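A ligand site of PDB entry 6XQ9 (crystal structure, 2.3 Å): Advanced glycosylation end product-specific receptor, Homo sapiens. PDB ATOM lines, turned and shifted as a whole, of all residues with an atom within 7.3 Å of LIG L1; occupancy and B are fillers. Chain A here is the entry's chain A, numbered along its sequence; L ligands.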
ATOM      1  N   GLY A   1      -8.083 -25.411   8.447  1.00  0.00           N
ATOM      2  CA  GLY A   1      -6.755 -25.730   7.968  1.00  0.00           C
ATOM      3  C   GLY A   1      -5.683 -25.583   9.028  1.00  0.00           C
ATOM      4  O   GLY A   1      -5.900 -25.906  10.194  1.00  0.00           O
ATOM      5  N   ALA A   2      -4.504 -25.113   8.617  1.00  0.00           N
ATOM      6  CA  ALA A   2      -3.362 -24.950   9.491  1.00  0.00           C
ATOM      7  C   ALA A   2      -3.151 -23.482   9.829  1.00  0.00           C
ATOM      8  O   ALA A   2      -3.830 -22.595   9.284  1.00  0.00           O
ATOM      9  CB  ALA A   2      -2.099 -25.542   8.852  1.00  0.00           C
ATOM     10  N   MET A   3      -2.218 -23.220  10.737  1.00  0.00           N
ATOM     11  CA  MET A   3      -1.856 -21.844  11.051  1.00  0.00           C
ATOM     12  C   MET A   3      -1.244 -21.168   9.837  1.00  0.00           C
ATOM     13  O   MET A   3      -0.283 -21.676   9.252  1.00  0.00           O
ATOM     14  CB  MET A   3      -0.901 -21.785  12.248  1.00  0.00           C
ATOM     15  CG  MET A   3      -1.641 -21.885  13.551  1.00  0.00           C
ATOM     16  SD  MET A   3      -2.355 -20.299  14.081  1.00  0.00           S
ATOM     17  CE  MET A   3      -3.145 -20.875  15.596  1.00  0.00           C
ATOM     18  N   ALA A   4      -1.810 -20.034   9.448  1.00  0.00           N
ATOM     19  CA  ALA A   4      -1.359 -19.340   8.262  1.00  0.00           C
ATOM     20  C   ALA A   4      -1.305 -17.849   8.523  1.00  0.00           C
ATOM     21  O   ALA A   4      -1.944 -17.323   9.438  1.00  0.00           O
ATOM     22  CB  ALA A   4      -2.291 -19.621   7.067  1.00  0.00           C
ATOM     23  N   LEU A  30      13.327 -26.195  -2.887  1.00  0.00           N
ATOM     24  CA  LEU A  30      12.107 -25.622  -2.361  1.00  0.00           C
ATOM     25  C   LEU A  30      10.966 -26.000  -3.294  1.00  0.00           C
ATOM     26  O   LEU A  30      11.159 -26.310  -4.469  1.00  0.00           O
ATOM     27  CB  LEU A  30      12.216 -24.102  -2.196  1.00  0.00           C
ATOM     28  CG  LEU A  30      12.358 -23.207  -3.434  1.00  0.00           C
ATOM     29  CD1 LEU A  30      10.977 -22.854  -4.004  1.00  0.00           C
ATOM     30  CD2 LEU A  30      13.224 -21.971  -3.198  1.00  0.00           C
ATOM     31  N   GLU A  31       9.752 -25.934  -2.751  1.00  0.00           N
ATOM     32  CA  GLU A  31       8.567 -26.339  -3.488  1.00  0.00           C
ATOM     33  C   GLU A  31       7.394 -25.491  -3.042  1.00  0.00           C
ATOM     34  O   GLU A  31       7.197 -25.303  -1.831  1.00  0.00           O
ATOM     35  CB  GLU A  31       8.279 -27.821  -3.227  1.00  0.00           C
ATOM     36  CG  GLU A  31       7.281 -28.477  -4.140  1.00  0.00           C
ATOM     37  CD  GLU A  31       7.208 -29.977  -3.897  1.00  0.00           C
ATOM     38  OE1 GLU A  31       6.632 -30.380  -2.863  1.00  0.00           O
ATOM     39  OE2 GLU A  31       7.739 -30.747  -4.720  1.00  0.00           O
ATOM     40  N   TRP A  32       6.608 -25.004  -4.000  1.00  0.00           N
ATOM     41  CA  TRP A  32       5.410 -24.227  -3.725  1.00  0.00           C
ATOM     42  C   TRP A  32       4.222 -25.125  -4.044  1.00  0.00           C
ATOM     43  O   TRP A  32       4.240 -25.839  -5.050  1.00  0.00           O
ATOM     44  CB  TRP A  32       5.387 -22.943  -4.562  1.00  0.00           C
ATOM     45  CG  TRP A  32       6.093 -21.771  -3.907  1.00  0.00           C
ATOM     46  CD1 TRP A  32       7.362 -21.335  -4.159  1.00  0.00           C
ATOM     47  CD2 TRP A  32       5.554 -20.861  -2.933  1.00  0.00           C
ATOM     48  NE1 TRP A  32       7.648 -20.239  -3.392  1.00  0.00           N
ATOM     49  CE2 TRP A  32       6.563 -19.920  -2.634  1.00  0.00           C
ATOM     50  CE3 TRP A  32       4.316 -20.761  -2.280  1.00  0.00           C
ATOM     51  CZ2 TRP A  32       6.370 -18.888  -1.701  1.00  0.00           C
ATOM     52  CZ3 TRP A  32       4.138 -19.732  -1.363  1.00  0.00           C
ATOM     53  CH2 TRP A  32       5.156 -18.812  -1.083  1.00  0.00           C
ATOM     54  N   LYS A  33       3.237 -25.149  -3.155  1.00  0.00           N
ATOM     55  CA  LYS A  33       1.972 -25.834  -3.367  1.00  0.00           C
ATOM     56  C   LYS A  33       0.863 -24.814  -3.200  1.00  0.00           C
ATOM     57  O   LYS A  33       0.858 -24.054  -2.241  1.00  0.00           O
ATOM     58  CB  LYS A  33       1.814 -27.016  -2.379  1.00  0.00           C
ATOM     59  CG  LYS A  33       2.594 -28.257  -2.799  1.00  0.00           C
ATOM     60  CD  LYS A  33       2.918 -29.206  -1.629  1.00  0.00           C
ATOM     61  CE  LYS A  33       1.764 -30.014  -1.094  1.00  0.00           C
ATOM     62  NZ  LYS A  33       2.302 -31.281  -0.485  1.00  0.00           N
ATOM     63  N   LEU A  34      -0.070 -24.784  -4.130  1.00  0.00           N
ATOM     64  CA  LEU A  34      -1.180 -23.854  -3.999  1.00  0.00           C
ATOM     65  C   LEU A  34      -2.495 -24.550  -4.304  1.00  0.00           C
ATOM     66  O   LEU A  34      -2.558 -25.482  -5.102  1.00  0.00           O
ATOM     67  CB  LEU A  34      -0.975 -22.600  -4.872  1.00  0.00           C
ATOM     68  CG  LEU A  34      -1.166 -22.628  -6.378  1.00  0.00           C
ATOM     69  CD1 LEU A  34      -1.303 -21.206  -6.889  1.00  0.00           C
ATOM     70  CD2 LEU A  34       0.026 -23.300  -7.034  1.00  0.00           C
ATOM     71  N   TRP A  42      -4.420 -29.427  -4.904  1.00  0.00           N
ATOM     72  CA  TRP A  42      -3.084 -28.852  -4.830  1.00  0.00           C
ATOM     73  C   TRP A  42      -2.373 -28.895  -6.181  1.00  0.00           C
ATOM     74  O   TRP A  42      -2.389 -29.926  -6.870  1.00  0.00           O
ATOM     75  CB  TRP A  42      -2.230 -29.579  -3.792  1.00  0.00           C
ATOM     76  CG  TRP A  42      -2.660 -29.285  -2.406  1.00  0.00           C
ATOM     77  CD1 TRP A  42      -3.351 -30.115  -1.598  1.00  0.00           C
ATOM     78  CD2 TRP A  42      -2.463 -28.068  -1.667  1.00  0.00           C
ATOM     79  NE1 TRP A  42      -3.594 -29.514  -0.400  1.00  0.00           N
ATOM     80  CE2 TRP A  42      -3.059 -28.251  -0.420  1.00  0.00           C
ATOM     81  CE3 TRP A  42      -1.835 -26.860  -1.954  1.00  0.00           C
ATOM     82  CZ2 TRP A  42      -3.045 -27.269   0.575  1.00  0.00           C
ATOM     83  CZ3 TRP A  42      -1.826 -25.873  -0.971  1.00  0.00           C
ATOM     84  CH2 TRP A  42      -2.432 -26.085   0.271  1.00  0.00           C
ATOM     85  N   VAL A  44       1.552 -28.060  -7.729  1.00  0.00           N
ATOM     86  CA  VAL A  44       2.945 -27.900  -7.318  1.00  0.00           C
ATOM     87  C   VAL A  44       3.669 -27.027  -8.336  1.00  0.00           C
ATOM     88  O   VAL A  44       3.593 -27.271  -9.541  1.00  0.00           O
ATOM     89  CB  VAL A  44       3.640 -29.274  -7.188  1.00  0.00           C
ATOM     90  CG1 VAL A  44       5.139 -29.108  -7.111  1.00  0.00           C
ATOM     91  CG2 VAL A  44       3.111 -30.021  -5.968  1.00  0.00           C
ATOM     92  N   PHE A  78      -1.546 -20.802  -0.233  1.00  0.00           N
ATOM     93  CA  PHE A  78      -0.212 -20.856  -0.850  1.00  0.00           C
ATOM     94  C   PHE A  78       0.789 -21.315   0.207  1.00  0.00           C
ATOM     95  O   PHE A  78       0.896 -20.695   1.266  1.00  0.00           O
ATOM     96  CB  PHE A  78       0.202 -19.488  -1.410  1.00  0.00           C
ATOM     97  CG  PHE A  78      -0.674 -18.957  -2.516  1.00  0.00           C
ATOM     98  CD1 PHE A  78      -0.171 -18.811  -3.797  1.00  0.00           C
ATOM     99  CD2 PHE A  78      -1.982 -18.565  -2.271  1.00  0.00           C
ATOM    100  CE1 PHE A  78      -0.960 -18.303  -4.819  1.00  0.00           C
ATOM    101  CE2 PHE A  78      -2.776 -18.044  -3.295  1.00  0.00           C
ATOM    102  CZ  PHE A  78      -2.263 -17.914  -4.562  1.00  0.00           C
ATOM    103  N   ARG A  79       1.520 -22.389  -0.076  1.00  0.00           N
ATOM    104  CA  ARG A  79       2.489 -22.946   0.860  1.00  0.00           C
ATOM    105  C   ARG A  79       3.845 -23.142   0.215  1.00  0.00           C
ATOM    106  O   ARG A  79       3.946 -23.573  -0.933  1.00  0.00           O
ATOM    107  CB  ARG A  79       2.066 -24.293   1.375  1.00  0.00           C
ATOM    108  CG  ARG A  79       0.977 -24.243   2.357  1.00  0.00           C
ATOM    109  CD  ARG A  79       0.352 -25.582   2.449  1.00  0.00           C
ATOM    110  NE  ARG A  79      -0.659 -25.600   3.488  1.00  0.00           N
ATOM    111  CZ  ARG A  79      -1.061 -26.701   4.093  1.00  0.00           C
ATOM    112  NH1 ARG A  79      -0.538 -27.875   3.743  1.00  0.00           N
ATOM    113  NH2 ARG A  79      -1.988 -26.625   5.028  1.00  0.00           N
ATOM    114  N   CYS A  80       4.890 -22.873   0.972  1.00  0.00           N
ATOM    115  CA  CYS A  80       6.247 -23.167   0.536  1.00  0.00           C
ATOM    116  C   CYS A  80       6.895 -24.095   1.546  1.00  0.00           C
ATOM    117  O   CYS A  80       6.622 -24.019   2.747  1.00  0.00           O
ATOM    118  CB  CYS A  80       7.099 -21.884   0.375  1.00  0.00           C
ATOM    119  SG  CYS A  80       8.572 -22.119  -0.687  1.00  0.00           S
ATOM    120  N   GLN A  81       7.743 -24.983   1.045  1.00  0.00           N
ATOM    121  CA  GLN A  81       8.593 -25.814   1.876  1.00  0.00           C
ATOM    122  C   GLN A  81       9.991 -25.744   1.286  1.00  0.00           C
ATOM    123  O   GLN A  81      10.176 -26.027   0.099  1.00  0.00           O
ATOM    124  CB  GLN A  81       8.099 -27.261   1.958  1.00  0.00           C
ATOM    125  N   ALA A  82      10.972 -25.379   2.109  1.00  0.00           N
ATOM    126  CA  ALA A  82      12.336 -25.176   1.639  1.00  0.00           C
ATOM    127  C   ALA A  82      13.316 -25.818   2.608  1.00  0.00           C
ATOM    128  O   ALA A  82      13.041 -25.954   3.802  1.00  0.00           O
ATOM    129  CB  ALA A  82      12.642 -23.683   1.469  1.00  0.00           C
ATOM    130  N   GLU A  89      14.362 -27.935   7.432  1.00  0.00           N
ATOM    131  CA  GLU A  89      13.181 -27.656   6.623  1.00  0.00           C
ATOM    132  C   GLU A  89      12.388 -26.505   7.238  1.00  0.00           C
ATOM    133  O   GLU A  89      12.170 -26.473   8.458  1.00  0.00           O
ATOM    134  CB  GLU A  89      12.310 -28.910   6.513  1.00  0.00           C
ATOM    135  CG  GLU A  89      12.956 -30.050   5.750  1.00  0.00           C
ATOM    136  CD  GLU A  89      11.945 -31.061   5.214  1.00  0.00           C
ATOM    137  OE1 GLU A  89      12.373 -32.079   4.632  1.00  0.00           O
ATOM    138  OE2 GLU A  89      10.726 -30.826   5.379  1.00  0.00           O
ATOM    139  N   THR A  90      11.954 -25.571   6.400  1.00  0.00           N
ATOM    140  CA  THR A  90      11.128 -24.452   6.811  1.00  0.00           C
ATOM    141  C   THR A  90       9.861 -24.403   5.952  1.00  0.00           C
ATOM    142  O   THR A  90       9.920 -24.605   4.733  1.00  0.00           O
ATOM    143  CB  THR A  90      11.892 -23.125   6.694  1.00  0.00           C
ATOM    144  OG1 THR A  90      13.207 -23.292   7.246  1.00  0.00           O
ATOM    145  CG2 THR A  90      11.164 -22.029   7.447  1.00  0.00           C
ATOM    146  N   LYS A  91       8.737 -24.106   6.600  1.00  0.00           N
ATOM    147  CA  LYS A  91       7.444 -24.050   5.956  1.00  0.00           C
ATOM    148  C   LYS A  91       6.853 -22.651   6.045  1.00  0.00           C
ATOM    149  O   LYS A  91       7.050 -21.946   7.043  1.00  0.00           O
ATOM    150  CB  LYS A  91       6.466 -25.060   6.569  1.00  0.00           C
ATOM    151  CG  LYS A  91       6.780 -26.521   6.261  1.00  0.00           C
ATOM    152  CD  LYS A  91       5.728 -27.440   6.863  1.00  0.00           C
ATOM    153  CE  LYS A  91       5.626 -28.750   6.101  1.00  0.00           C
ATOM    154  NZ  LYS A  91       6.668 -29.716   6.551  1.00  0.00           N
ATOM    155  N   SER A  92       6.128 -22.257   5.000  1.00  0.00           N
ATOM    156  CA  SER A  92       5.434 -20.978   4.920  1.00  0.00           C
ATOM    157  C   SER A  92       4.007 -21.236   4.462  1.00  0.00           C
ATOM    158  O   SER A  92       3.795 -21.889   3.439  1.00  0.00           O
ATOM    159  CB  SER A  92       6.141 -20.021   3.952  1.00  0.00           C
ATOM    160  OG  SER A  92       7.477 -19.755   4.356  1.00  0.00           O
ATOM    161  N   ASN A  93       3.040 -20.720   5.205  1.00  0.00           N
ATOM    162  CA  ASN A  93       1.621 -20.981   4.952  1.00  0.00           C
ATOM    163  C   ASN A  93       0.868 -19.659   4.863  1.00  0.00           C
ATOM    164  O   ASN A  93       0.875 -18.871   5.817  1.00  0.00           O
ATOM    165  CB  ASN A  93       1.046 -21.878   6.065  1.00  0.00           C
ATOM    166  CG  ASN A  93      -0.277 -22.516   5.685  1.00  0.00           C
ATOM    167  OD1 ASN A  93      -0.546 -22.785   4.516  1.00  0.00           O
ATOM    168  ND2 ASN A  93      -1.114 -22.781   6.683  1.00  0.00           N
ATOM    169  N   TYR A  94       0.214 -19.424   3.722  1.00  0.00           N
ATOM    170  CA  TYR A  94      -0.464 -18.162   3.445  1.00  0.00           C
ATOM    171  C   TYR A  94      -1.898 -18.435   3.026  1.00  0.00           C
ATOM    172  O   TYR A  94      -2.148 -19.307   2.184  1.00  0.00           O
ATOM    173  CB  TYR A  94       0.238 -17.382   2.320  1.00  0.00           C
ATOM    174  CG  TYR A  94       1.678 -17.015   2.606  1.00  0.00           C
ATOM    175  CD1 TYR A  94       1.986 -15.935   3.423  1.00  0.00           C
ATOM    176  CD2 TYR A  94       2.717 -17.735   2.042  1.00  0.00           C
ATOM    177  CE1 TYR A  94       3.305 -15.585   3.675  1.00  0.00           C
ATOM    178  CE2 TYR A  94       4.037 -17.394   2.283  1.00  0.00           C
ATOM    179  CZ  TYR A  94       4.329 -16.320   3.105  1.00  0.00           C
ATOM    180  OH  TYR A  94       5.637 -15.985   3.342  1.00  0.00           O
HETATM  181  C1  LIG L   1       2.631 -29.441   4.022  1.00  0.00           C
HETATM  182  C2  LIG L   1       3.319 -28.363   3.477  1.00  0.00           C
HETATM  183  C3  LIG L   1       3.090 -27.277   4.281  1.00  0.00           C
HETATM  184  C4  LIG L   1       2.251 -27.685   5.316  1.00  0.00           C
HETATM  185  C5  LIG L   1       2.577 -30.867   3.477  1.00  0.00           C
HETATM  186  C6  LIG L   1       4.193 -28.402   2.216  1.00  0.00           C
HETATM  187  C7  LIG L   1       1.782 -26.682   6.425  1.00  0.00           C
HETATM  188  C8  LIG L   1       3.576 -25.777   4.219  1.00  0.00           C
HETATM  189  C9  LIG L   1       3.126 -24.794   5.281  1.00  0.00           C
HETATM  190  C10 LIG L   1       2.235 -25.248   6.381  1.00  0.00           C
HETATM  191  C11 LIG L   1       0.860 -27.171   7.544  1.00  0.00           C
HETATM  192  C12 LIG L   1       4.206 -27.245   1.228  1.00  0.00           C
HETATM  193  C13 LIG L   1       5.068 -29.623   1.937  1.00  0.00           C
HETATM  194  C14 LIG L   1       5.950 -29.688   0.689  1.00  0.00           C
HETATM  195  C15 LIG L   1       5.082 -27.297  -0.022  1.00  0.00           C
HETATM  196  C16 LIG L   1       5.951 -28.528  -0.292  1.00  0.00           C
HETATM  197  N1  LIG L   1       1.973 -29.016   5.139  1.00  0.00           N
HETATM  198  O1  LIG L   1       3.059 -31.815   4.161  1.00  0.00           O
HETATM  199  O2  LIG L   1       2.064 -31.089   2.349  1.00  0.00           O
HETATM  200  C1  LG2 L   2      10.228 -30.537   1.042  1.00  0.00           C
HETATM  201  C2  LG2 L   2       9.691 -31.113  -0.096  1.00  0.00           C
HETATM  202  C3  LG2 L   2      10.086 -30.677  -1.354  1.00  0.00           C
HETATM  203  C4  LG2 L   2      11.027 -29.659  -1.459  1.00  0.00           C
HETATM  204  C5  LG2 L   2      11.553 -29.080  -0.315  1.00  0.00           C
HETATM  205  C6  LG2 L   2      11.158 -29.525   0.931  1.00  0.00           C
HETATM  206  C7  LG2 L   2      12.566 -29.895  -3.200  1.00  0.00           C
HETATM  207  C8  LG2 L   2      13.039 -29.581  -4.465  1.00  0.00           C
HETATM  208  C9  LG2 L   2      14.162 -30.223  -4.954  1.00  0.00           C
HETATM  209  C10 LG2 L   2      14.800 -31.185  -4.183  1.00  0.00           C
HETATM  210  C11 LG2 L   2      14.330 -31.499  -2.927  1.00  0.00           C
HETATM  211  C12 LG2 L   2      13.207 -30.857  -2.438  1.00  0.00           C
HETATM  212  C13 LG2 L   2      16.032 -31.897  -4.741  1.00  0.00           C
HETATM  213  O1  LG2 L   2      11.429 -29.213  -2.725  1.00  0.00           O
HETATM  214  O2  LG2 L   2      16.312 -31.779  -5.966  1.00  0.00           O
HETATM  215  O3  LG2 L   2      11.696 -28.940   2.080  1.00  0.00           O
HETATM  216  O4  LG2 L   2      16.763 -32.580  -3.980  1.00  0.00           O
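The guanidinium group (NH1) of Arg 79 sits close to a nitrogen (N1) of LIG L1 (3.1 Å). An oxygen (O2) of LIG L1 is in salt-bridge range of the side-chain amino group (NZ) of Lys 33 (2.9 Å).
The backbone NH (N) of Glu 31 lies within hydrogen-bond range of the backbone carbonyl oxygen (O) of Gln 81, 2.9 Å away. The indole nitrogen (NE1) of Trp 32 sits at hydrogen-bond distance from the side-chain sulfur (SG) of Cys 80 (3.4 Å). ND2 of Asn 93 lies within hydrogen-bond range of O of Met 3 (2.9 Å). The backbone carbonyl oxygen of Lys 33 is in hydrogen-bond range of the backbone NH of Arg 79, at 2.8 Å. NE of Arg 79 lies within hydrogen-bond range of OD1 of Asn 93 (3.0 Å). The backbone NH (N) of Cys 80 is in hydrogen-bond range of the backbone carbonyl oxygen (O) of Ser 92 (2.9 Å).
Ala 2 touches LIG L1. Glu 31 touches LIG L1 (OE1 to C16, 3.2 Å). Cys 80 touches LIG L1 (O to C8, 3.8 Å). Gln 81 touches LIG L1. Lys 91 touches LIG L1. Ser 92 touches LIG L1. Asn 93 touches LIG L1 (CB to C10, 3.6 Å). Nine residues have an atom within 4 Å of LIG L1: Ala 2, Glu 31, Lys 33, Arg 79, Cys 80, Gln 81, Lys 91, Ser 92 and Asn 93. The nearest printed residue that does not touch LIG L1 is Trp 32 (4.7 Å).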
